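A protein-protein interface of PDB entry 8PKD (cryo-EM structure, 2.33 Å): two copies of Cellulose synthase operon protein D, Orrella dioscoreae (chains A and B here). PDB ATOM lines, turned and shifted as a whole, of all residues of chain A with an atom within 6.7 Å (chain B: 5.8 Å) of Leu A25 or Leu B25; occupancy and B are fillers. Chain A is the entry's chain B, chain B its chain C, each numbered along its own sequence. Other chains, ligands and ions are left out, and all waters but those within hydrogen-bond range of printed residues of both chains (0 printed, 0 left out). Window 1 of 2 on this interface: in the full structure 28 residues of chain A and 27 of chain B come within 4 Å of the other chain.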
ATOM      1  N   ALA A  17      12.376 -29.794  26.973  1.00  0.00           N
ATOM      2  CA  ALA A  17      12.120 -28.901  25.858  1.00  0.00           C
ATOM      3  C   ALA A  17      12.332 -29.633  24.534  1.00  0.00           C
ATOM      4  O   ALA A  17      13.161 -30.541  24.446  1.00  0.00           O
ATOM      5  CB  ALA A  17      13.035 -27.684  25.929  1.00  0.00           C
ATOM      6  N   GLN A  20      13.298 -28.366  18.664  1.00  0.00           N
ATOM      7  CA  GLN A  20      13.178 -27.156  17.861  1.00  0.00           C
ATOM      8  C   GLN A  20      13.733 -25.933  18.576  1.00  0.00           C
ATOM      9  O   GLN A  20      14.207 -24.999  17.920  1.00  0.00           O
ATOM     10  CB  GLN A  20      11.717 -26.924  17.478  1.00  0.00           C
ATOM     11  CG  GLN A  20      11.523 -25.991  16.300  1.00  0.00           C
ATOM     12  CD  GLN A  20      10.065 -25.728  16.000  1.00  0.00           C
ATOM     13  OE1 GLN A  20       9.571 -26.064  14.924  1.00  0.00           O
ATOM     14  NE2 GLN A  20       9.363 -25.130  16.951  1.00  0.00           N
ATOM     15  N   TRP A  21      13.693 -25.915  19.906  1.00  0.00           N
ATOM     16  CA  TRP A  21      14.011 -24.711  20.654  1.00  0.00           C
ATOM     17  C   TRP A  21      15.119 -24.871  21.682  1.00  0.00           C
ATOM     18  O   TRP A  21      15.523 -23.866  22.275  1.00  0.00           O
ATOM     19  CB  TRP A  21      12.755 -24.181  21.358  1.00  0.00           C
ATOM     20  CG  TRP A  21      11.800 -23.548  20.417  1.00  0.00           C
ATOM     21  CD1 TRP A  21      10.629 -24.071  19.965  1.00  0.00           C
ATOM     22  CD2 TRP A  21      11.940 -22.274  19.787  1.00  0.00           C
ATOM     23  NE1 TRP A  21      10.024 -23.196  19.099  1.00  0.00           N
ATOM     24  CE2 TRP A  21      10.812 -22.085  18.972  1.00  0.00           C
ATOM     25  CE3 TRP A  21      12.912 -21.271  19.837  1.00  0.00           C
ATOM     26  CZ2 TRP A  21      10.627 -20.935  18.212  1.00  0.00           C
ATOM     27  CZ3 TRP A  21      12.727 -20.133  19.085  1.00  0.00           C
ATOM     28  CH2 TRP A  21      11.596 -19.974  18.283  1.00  0.00           C
ATOM     29  N   ARG A  22      15.627 -26.081  21.906  1.00  0.00           N
ATOM     30  CA  ARG A  22      16.626 -26.278  22.951  1.00  0.00           C
ATOM     31  C   ARG A  22      17.878 -25.455  22.675  1.00  0.00           C
ATOM     32  O   ARG A  22      18.322 -24.670  23.524  1.00  0.00           O
ATOM     33  CB  ARG A  22      16.968 -27.763  23.066  1.00  0.00           C
ATOM     34  CG  ARG A  22      17.867 -28.105  24.235  1.00  0.00           C
ATOM     35  CD  ARG A  22      18.172 -29.592  24.287  1.00  0.00           C
ATOM     36  NE  ARG A  22      16.974 -30.400  24.475  1.00  0.00           N
ATOM     37  CZ  ARG A  22      16.493 -31.244  23.573  1.00  0.00           C
ATOM     38  NH1 ARG A  22      17.100 -31.435  22.413  1.00  0.00           N
ATOM     39  NH2 ARG A  22      15.380 -31.918  23.843  1.00  0.00           N
ATOM     40  N   GLY A  23      18.444 -25.595  21.476  1.00  0.00           N
ATOM     41  CA  GLY A  23      19.658 -24.866  21.150  1.00  0.00           C
ATOM     42  C   GLY A  23      19.447 -23.367  21.067  1.00  0.00           C
ATOM     43  O   GLY A  23      20.286 -22.587  21.525  1.00  0.00           O
ATOM     44  N   ALA A  24      18.329 -22.943  20.474  1.00  0.00           N
ATOM     45  CA  ALA A  24      18.054 -21.515  20.358  1.00  0.00           C
ATOM     46  C   ALA A  24      17.907 -20.866  21.726  1.00  0.00           C
ATOM     47  O   ALA A  24      18.471 -19.794  21.978  1.00  0.00           O
ATOM     48  CB  ALA A  24      16.797 -21.291  19.520  1.00  0.00           C
ATOM     49  N   LEU A  25      17.166 -21.506  22.633  1.00  0.00           N
ATOM     50  CA  LEU A  25      16.999 -20.944  23.964  1.00  0.00           C
ATOM     51  C   LEU A  25      18.292 -21.005  24.763  1.00  0.00           C
ATOM     52  O   LEU A  25      18.562 -20.105  25.564  1.00  0.00           O
ATOM     53  CB  LEU A  25      15.866 -21.662  24.695  1.00  0.00           C
ATOM     54  CG  LEU A  25      14.477 -21.375  24.123  1.00  0.00           C
ATOM     55  CD1 LEU A  25      13.388 -21.888  25.043  1.00  0.00           C
ATOM     56  CD2 LEU A  25      14.301 -19.889  23.862  1.00  0.00           C
ATOM     57  N   GLY A  26      19.111 -22.038  24.557  1.00  0.00           N
ATOM     58  CA  GLY A  26      20.414 -22.060  25.197  1.00  0.00           C
ATOM     59  C   GLY A  26      21.297 -20.914  24.743  1.00  0.00           C
ATOM     60  O   GLY A  26      21.973 -20.276  25.554  1.00  0.00           O
ATOM     61  N   ALA A  27      21.296 -20.634  23.440  1.00  0.00           N
ATOM     62  CA  ALA A  27      22.072 -19.513  22.923  1.00  0.00           C
ATOM     63  C   ALA A  27      21.548 -18.185  23.455  1.00  0.00           C
ATOM     64  O   ALA A  27      22.331 -17.289  23.799  1.00  0.00           O
ATOM     65  CB  ALA A  27      22.051 -19.528  21.396  1.00  0.00           C
ATOM     66  N   LEU A  28      20.224 -18.038  23.524  1.00  0.00           N
ATOM     67  CA  LEU A  28      19.648 -16.814  24.069  1.00  0.00           C
ATOM     68  C   LEU A  28      20.025 -16.637  25.533  1.00  0.00           C
ATOM     69  O   LEU A  28      20.331 -15.524  25.975  1.00  0.00           O
ATOM     70  CB  LEU A  28      18.132 -16.828  23.897  1.00  0.00           C
ATOM     71  CG  LEU A  28      17.370 -15.625  24.449  1.00  0.00           C
ATOM     72  CD1 LEU A  28      17.854 -14.345  23.796  1.00  0.00           C
ATOM     73  CD2 LEU A  28      15.882 -15.804  24.230  1.00  0.00           C
ATOM     74  N   ALA A  29      20.013 -17.728  26.302  1.00  0.00           N
ATOM     75  CA  ALA A  29      20.422 -17.657  27.699  1.00  0.00           C
ATOM     76  C   ALA A  29      21.891 -17.282  27.820  1.00  0.00           C
ATOM     77  O   ALA A  29      22.270 -16.515  28.712  1.00  0.00           O
ATOM     78  CB  ALA A  29      20.146 -18.988  28.396  1.00  0.00           C
ATOM     79  N   GLN A  30      22.734 -17.823  26.941  1.00  0.00           N
ATOM     80  CA  GLN A  30      24.147 -17.461  26.960  1.00  0.00           C
ATOM     81  C   GLN A  30      24.336 -15.975  26.692  1.00  0.00           C
ATOM     82  O   GLN A  30      25.120 -15.305  27.376  1.00  0.00           O
ATOM     83  CB  GLN A  30      24.917 -18.294  25.938  1.00  0.00           C
ATOM     84  CG  GLN A  30      26.415 -18.071  25.966  1.00  0.00           C
ATOM     85  CD  GLN A  30      27.108 -18.911  27.014  1.00  0.00           C
ATOM     86  OE1 GLN A  30      27.770 -18.386  27.907  1.00  0.00           O
ATOM     87  NE2 GLN A  30      26.963 -20.225  26.909  1.00  0.00           N
ATOM     88  N   PHE A  52       2.897 -13.657  31.624  1.00  0.00           N
ATOM     89  CA  PHE A  52       2.354 -14.977  31.318  1.00  0.00           C
ATOM     90  C   PHE A  52       1.120 -15.272  32.158  1.00  0.00           C
ATOM     91  O   PHE A  52       0.128 -15.806  31.651  1.00  0.00           O
ATOM     92  CB  PHE A  52       3.423 -16.046  31.539  1.00  0.00           C
ATOM     93  CG  PHE A  52       2.932 -17.451  31.342  1.00  0.00           C
ATOM     94  CD1 PHE A  52       2.462 -18.192  32.410  1.00  0.00           C
ATOM     95  CD2 PHE A  52       2.947 -18.033  30.090  1.00  0.00           C
ATOM     96  CE1 PHE A  52       2.014 -19.482  32.231  1.00  0.00           C
ATOM     97  CE2 PHE A  52       2.501 -19.322  29.907  1.00  0.00           C
ATOM     98  CZ  PHE A  52       2.034 -20.047  30.977  1.00  0.00           C
ATOM     99  N   TRP A  80       4.007 -28.045  31.817  1.00  0.00           N
ATOM    100  CA  TRP A  80       4.921 -27.272  32.647  1.00  0.00           C
ATOM    101  C   TRP A  80       4.958 -27.767  34.088  1.00  0.00           C
ATOM    102  O   TRP A  80       5.079 -26.967  35.021  1.00  0.00           O
ATOM    103  CB  TRP A  80       4.550 -25.791  32.606  1.00  0.00           C
ATOM    104  CG  TRP A  80       5.301 -25.001  31.589  1.00  0.00           C
ATOM    105  CD1 TRP A  80       5.149 -25.046  30.241  1.00  0.00           C
ATOM    106  CD2 TRP A  80       6.317 -24.027  31.846  1.00  0.00           C
ATOM    107  NE1 TRP A  80       6.014 -24.170  29.636  1.00  0.00           N
ATOM    108  CE2 TRP A  80       6.742 -23.531  30.604  1.00  0.00           C
ATOM    109  CE3 TRP A  80       6.910 -23.530  33.008  1.00  0.00           C
ATOM    110  CZ2 TRP A  80       7.732 -22.563  30.487  1.00  0.00           C
ATOM    111  CZ3 TRP A  80       7.894 -22.573  32.891  1.00  0.00           C
ATOM    112  CH2 TRP A  80       8.295 -22.098  31.641  1.00  0.00           C
ATOM    113  N   SER A 103      15.723 -27.537  30.970  1.00  0.00           N
ATOM    114  CA  SER A 103      15.980 -28.085  29.644  1.00  0.00           C
ATOM    115  C   SER A 103      16.233 -26.981  28.629  1.00  0.00           C
ATOM    116  O   SER A 103      17.020 -27.157  27.691  1.00  0.00           O
ATOM    117  CB  SER A 103      14.806 -28.957  29.201  1.00  0.00           C
ATOM    118  OG  SER A 103      14.992 -29.423  27.875  1.00  0.00           O
ATOM    119  N   ALA A 104      15.576 -25.836  28.797  1.00  0.00           N
ATOM    120  CA  ALA A 104      15.708 -24.754  27.830  1.00  0.00           C
ATOM    121  C   ALA A 104      16.955 -23.917  28.084  1.00  0.00           C
ATOM    122  O   ALA A 104      17.833 -23.823  27.219  1.00  0.00           O
ATOM    123  CB  ALA A 104      14.465 -23.870  27.862  1.00  0.00           C
ATOM    124  N   PHE A 105      17.049 -23.303  29.259  1.00  0.00           N
ATOM    125  CA  PHE A 105      18.100 -22.337  29.539  1.00  0.00           C
ATOM    126  C   PHE A 105      19.319 -22.943  30.216  1.00  0.00           C
ATOM    127  O   PHE A 105      20.272 -22.214  30.506  1.00  0.00           O
ATOM    128  CB  PHE A 105      17.545 -21.196  30.397  1.00  0.00           C
ATOM    129  CG  PHE A 105      16.352 -20.514  29.797  1.00  0.00           C
ATOM    130  CD1 PHE A 105      16.445 -19.876  28.576  1.00  0.00           C
ATOM    131  CD2 PHE A 105      15.138 -20.511  30.454  1.00  0.00           C
ATOM    132  CE1 PHE A 105      15.350 -19.250  28.023  1.00  0.00           C
ATOM    133  CE2 PHE A 105      14.040 -19.886  29.904  1.00  0.00           C
ATOM    134  CZ  PHE A 105      14.147 -19.256  28.688  1.00  0.00           C
ATOM    135  N   GLY A 106      19.322 -24.237  30.473  1.00  0.00           N
ATOM    136  CA  GLY A 106      20.468 -24.859  31.103  1.00  0.00           C
ATOM    137  C   GLY A 106      20.335 -24.906  32.612  1.00  0.00           C
ATOM    138  O   GLY A 106      19.680 -24.064  33.236  1.00  0.00           O
ATOM    139  N   ASN A 109      21.791 -21.953  34.726  1.00  0.00           N
ATOM    140  CA  ASN A 109      21.022 -20.719  34.678  1.00  0.00           C
ATOM    141  C   ASN A 109      19.780 -20.763  35.556  1.00  0.00           C
ATOM    142  O   ASN A 109      19.067 -19.756  35.651  1.00  0.00           O
ATOM    143  CB  ASN A 109      20.629 -20.405  33.235  1.00  0.00           C
ATOM    144  CG  ASN A 109      21.824 -20.066  32.373  1.00  0.00           C
ATOM    145  OD1 ASN A 109      22.740 -19.373  32.809  1.00  0.00           O
ATOM    146  ND2 ASN A 109      21.823 -20.554  31.140  1.00  0.00           N
ATOM    147  N   PHE A 116      11.088 -16.877  36.786  1.00  0.00           N
ATOM    148  CA  PHE A 116       9.886 -16.874  35.959  1.00  0.00           C
ATOM    149  C   PHE A 116       8.685 -17.372  36.749  1.00  0.00           C
ATOM    150  O   PHE A 116       7.632 -16.726  36.777  1.00  0.00           O
ATOM    151  CB  PHE A 116      10.112 -17.733  34.716  1.00  0.00           C
ATOM    152  CG  PHE A 116       8.915 -17.842  33.822  1.00  0.00           C
ATOM    153  CD1 PHE A 116       8.618 -16.841  32.918  1.00  0.00           C
ATOM    154  CD2 PHE A 116       8.095 -18.951  33.870  1.00  0.00           C
ATOM    155  CE1 PHE A 116       7.524 -16.942  32.090  1.00  0.00           C
ATOM    156  CE2 PHE A 116       7.000 -19.055  33.045  1.00  0.00           C
ATOM    157  CZ  PHE A 116       6.716 -18.050  32.154  1.00  0.00           C
ATOM    158  N   TRP B  21       5.957 -23.922  24.714  1.00  0.00           N
ATOM    159  CA  TRP B  21       6.789 -22.738  24.839  1.00  0.00           C
ATOM    160  C   TRP B  21       6.217 -21.484  24.199  1.00  0.00           C
ATOM    161  O   TRP B  21       6.818 -20.416  24.354  1.00  0.00           O
ATOM    162  CB  TRP B  21       8.179 -23.006  24.245  1.00  0.00           C
ATOM    163  CG  TRP B  21       9.010 -23.860  25.127  1.00  0.00           C
ATOM    164  CD1 TRP B  21       9.301 -25.176  24.952  1.00  0.00           C
ATOM    165  CD2 TRP B  21       9.651 -23.462  26.340  1.00  0.00           C
ATOM    166  NE1 TRP B  21      10.091 -25.625  25.981  1.00  0.00           N
ATOM    167  CE2 TRP B  21      10.319 -24.589  26.846  1.00  0.00           C
ATOM    168  CE3 TRP B  21       9.727 -22.260  27.045  1.00  0.00           C
ATOM    169  CZ2 TRP B  21      11.053 -24.551  28.026  1.00  0.00           C
ATOM    170  CZ3 TRP B  21      10.456 -22.223  28.213  1.00  0.00           C
ATOM    171  CH2 TRP B  21      11.109 -23.360  28.693  1.00  0.00           C
ATOM    172  N   ARG B  22       5.082 -21.568  23.507  1.00  0.00           N
ATOM    173  CA  ARG B  22       4.559 -20.397  22.811  1.00  0.00           C
ATOM    174  C   ARG B  22       4.244 -19.271  23.789  1.00  0.00           C
ATOM    175  O   ARG B  22       4.719 -18.140  23.628  1.00  0.00           O
ATOM    176  CB  ARG B  22       3.318 -20.782  22.007  1.00  0.00           C
ATOM    177  CG  ARG B  22       2.861 -19.711  21.038  1.00  0.00           C
ATOM    178  CD  ARG B  22       1.629 -20.144  20.267  1.00  0.00           C
ATOM    179  NE  ARG B  22       1.855 -21.371  19.515  1.00  0.00           N
ATOM    180  CZ  ARG B  22       1.214 -22.510  19.737  1.00  0.00           C
ATOM    181  NH1 ARG B  22       0.269 -22.602  20.656  1.00  0.00           N
ATOM    182  NH2 ARG B  22       1.520 -23.581  19.011  1.00  0.00           N
ATOM    183  N   GLY B  23       3.463 -19.570  24.828  1.00  0.00           N
ATOM    184  CA  GLY B  23       3.093 -18.540  25.785  1.00  0.00           C
ATOM    185  C   GLY B  23       4.272 -18.026  26.588  1.00  0.00           C
ATOM    186  O   GLY B  23       4.389 -16.821  26.832  1.00  0.00           O
ATOM    187  N   ALA B  24       5.157 -18.928  27.015  1.00  0.00           N
ATOM    188  CA  ALA B  24       6.318 -18.511  27.792  1.00  0.00           C
ATOM    189  C   ALA B  24       7.226 -17.596  26.982  1.00  0.00           C
ATOM    190  O   ALA B  24       7.685 -16.562  27.482  1.00  0.00           O
ATOM    191  CB  ALA B  24       7.088 -19.735  28.282  1.00  0.00           C
ATOM    192  N   LEU B  25       7.489 -17.951  25.722  1.00  0.00           N
ATOM    193  CA  LEU B  25       8.337 -17.112  24.890  1.00  0.00           C
ATOM    194  C   LEU B  25       7.653 -15.799  24.537  1.00  0.00           C
ATOM    195  O   LEU B  25       8.323 -14.767  24.438  1.00  0.00           O
ATOM    196  CB  LEU B  25       8.746 -17.872  23.631  1.00  0.00           C
ATOM    197  CG  LEU B  25       9.747 -19.000  23.883  1.00  0.00           C
ATOM    198  CD1 LEU B  25      10.274 -19.566  22.579  1.00  0.00           C
ATOM    199  CD2 LEU B  25      10.890 -18.510  24.753  1.00  0.00           C
ATOM    200  N   GLY B  26       6.331 -15.808  24.359  1.00  0.00           N
ATOM    201  CA  GLY B  26       5.626 -14.554  24.155  1.00  0.00           C
ATOM    202  C   GLY B  26       5.737 -13.629  25.351  1.00  0.00           C
ATOM    203  O   GLY B  26       5.952 -12.423  25.201  1.00  0.00           O
ATOM    204  N   ALA B  27       5.602 -14.183  26.556  1.00  0.00           N
ATOM    205  CA  ALA B  27       5.754 -13.377  27.763  1.00  0.00           C
ATOM    206  C   ALA B  27       7.175 -12.845  27.897  1.00  0.00           C
ATOM    207  O   ALA B  27       7.382 -11.687  28.286  1.00  0.00           O
ATOM    208  CB  ALA B  27       5.369 -14.200  28.989  1.00  0.00           C
ATOM    209  N   LEU B  28       8.169 -13.679  27.587  1.00  0.00           N
ATOM    210  CA  LEU B  28       9.555 -13.226  27.647  1.00  0.00           C
ATOM    211  C   LEU B  28       9.808 -12.106  26.649  1.00  0.00           C
ATOM    212  O   LEU B  28      10.498 -11.127  26.961  1.00  0.00           O
ATOM    213  CB  LEU B  28      10.499 -14.400  27.394  1.00  0.00           C
ATOM    214  CG  LEU B  28      11.993 -14.087  27.382  1.00  0.00           C
ATOM    215  CD1 LEU B  28      12.417 -13.476  28.702  1.00  0.00           C
ATOM    216  CD2 LEU B  28      12.788 -15.344  27.098  1.00  0.00           C
ATOM    217  N   ALA B  29       9.250 -12.226  25.442  1.00  0.00           N
ATOM    218  CA  ALA B  29       9.390 -11.169  24.450  1.00  0.00           C
ATOM    219  C   ALA B  29       8.708  -9.890  24.913  1.00  0.00           C
ATOM    220  O   ALA B  29       9.220  -8.789  24.685  1.00  0.00           O
ATOM    221  CB  ALA B  29       8.820 -11.627  23.109  1.00  0.00           C
ATOM    222  N   GLN B  30       7.545 -10.014  25.553  1.00  0.00           N
ATOM    223  CA  GLN B  30       6.866  -8.836  26.080  1.00  0.00           C
ATOM    224  C   GLN B  30       7.717  -8.132  27.125  1.00  0.00           C
ATOM    225  O   GLN B  30       7.849  -6.901  27.107  1.00  0.00           O
ATOM    226  CB  GLN B  30       5.513  -9.232  26.669  1.00  0.00           C
ATOM    227  CG  GLN B  30       4.690  -8.064  27.172  1.00  0.00           C
ATOM    228  CD  GLN B  30       3.943  -7.361  26.064  1.00  0.00           C
ATOM    229  OE1 GLN B  30       4.167  -6.180  25.804  1.00  0.00           O
ATOM    230  NE2 GLN B  30       3.048  -8.083  25.402  1.00  0.00           N
ATOM    231  N   ALA B 104       6.985 -17.822  17.989  1.00  0.00           N
ATOM    232  CA  ALA B 104       7.396 -17.750  19.385  1.00  0.00           C
ATOM    233  C   ALA B 104       7.255 -16.342  19.944  1.00  0.00           C
ATOM    234  O   ALA B 104       6.545 -16.127  20.932  1.00  0.00           O
ATOM    235  CB  ALA B 104       8.837 -18.233  19.532  1.00  0.00           C
ATOM    236  N   PHE B 105       7.922 -15.369  19.328  1.00  0.00           N
ATOM    237  CA  PHE B 105       7.981 -14.019  19.865  1.00  0.00           C
ATOM    238  C   PHE B 105       6.919 -13.092  19.295  1.00  0.00           C
ATOM    239  O   PHE B 105       6.881 -11.916  19.669  1.00  0.00           O
ATOM    240  CB  PHE B 105       9.371 -13.424  19.624  1.00  0.00           C
ATOM    241  CG  PHE B 105      10.486 -14.242  20.202  1.00  0.00           C
ATOM    242  CD1 PHE B 105      10.559 -14.468  21.562  1.00  0.00           C
ATOM    243  CD2 PHE B 105      11.457 -14.785  19.387  1.00  0.00           C
ATOM    244  CE1 PHE B 105      11.582 -15.221  22.096  1.00  0.00           C
ATOM    245  CE2 PHE B 105      12.483 -15.538  19.917  1.00  0.00           C
ATOM    246  CZ  PHE B 105      12.544 -15.756  21.273  1.00  0.00           C
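Of the 20 printed residues of chain A, 6 touch a printed residue of chain B.
Of the 12 printed residues of chain B, 6 touch a printed residue of chain A.
Printed residues of chain B that touch a printed residue of chain A: Trp B21, Gly B23, Ala B24, Leu B25, Ala B27 and Ala B104.
Hydrophobic or aromatic side chains of chain B within 4 Å of the printed part of chain A: Trp B21, Ala B24, Leu B25, Ala B27 and Ala B104.
Among the printed residues, 9 pairs touch across the chains.
Among the printed residues, no Asp or Glu carboxylate lies within 4 Å of a Lys or Arg side-chain nitrogen of the other chain.
Of chain B, only Leu B25 comes within 4 Å of Leu A25.
Of the printed residues of chain A, Leu B25 touches Leu A25.
Printed residues of chain A within 4 Å of Ala B27: Phe A52 (3.7 Å).
Of the printed residues of chain A, Gly B23 touches Phe A52.
Arg A22 touches none of the printed residues of chain B.
Gln B30 touches none of the printed residues of chain A.
The nearest residue of chain B that does not touch Leu A25 is Trp B21 (4.2 Å).
The nearest residue of chain A that does not touch Leu B25 is Trp A21 (4.2 Å).
The nearest printed residue of chain B that does not touch Trp A21 is Leu B25 (4.2 Å).
Ala A17 touches Trp B21 (CB to NE1, 3.6 Å).
Trp A21 touches Ala B104 (CH2 to CB, 3.5 Å).
Leu B25 touches Leu A25 (CD2 to CD2, 3.8 Å).
Phe A52 touches Gly B23 (CD2 to C, 3.7 Å).
Ala B24 touches Phe A52 (N to CD2, 3.9 Å).
CB of Ala B27 touches N of Phe A52, 3.7 Å away.
Trp A80 touches Trp B21.
CB of Ala B24 touches CZ2 of Trp A80, 3.6 Å away.
Ala A104 touches Trp B21 (CB to CZ2, 3.5 Å).
NH2 of Arg A22 is in hydrogen-bond range of O of Ala A17, 2.7 Å away.
N of Ala A17 sits at hydrogen-bond distance from OG of Ser A103 (2.8 Å).
NE1 of Trp A21 sits close to NE2 of Gln A20 (3.0 Å).
The backbone NH (N) of Gly A26 sits at hydrogen-bond distance from the backbone carbonyl oxygen (O) of Ala A104 (3.5 Å).
N of Gly B26 is in hydrogen-bond range of O of Ala B104, at 3.4 Å.
Trp A21 touches Ala B104, and with the chains exchanged Ala A104 touches Trp B21.
Leu B25 touches its own counterpart, Leu A25.
Positions printed for both chains: 21, 22, 23, 24, 25, 26, 27, 28, 29, 30, 104 and 105.
Of the 9 pairs that touch across the chains among the printed residues, 3 have their exchanged pair printed and touching as well.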
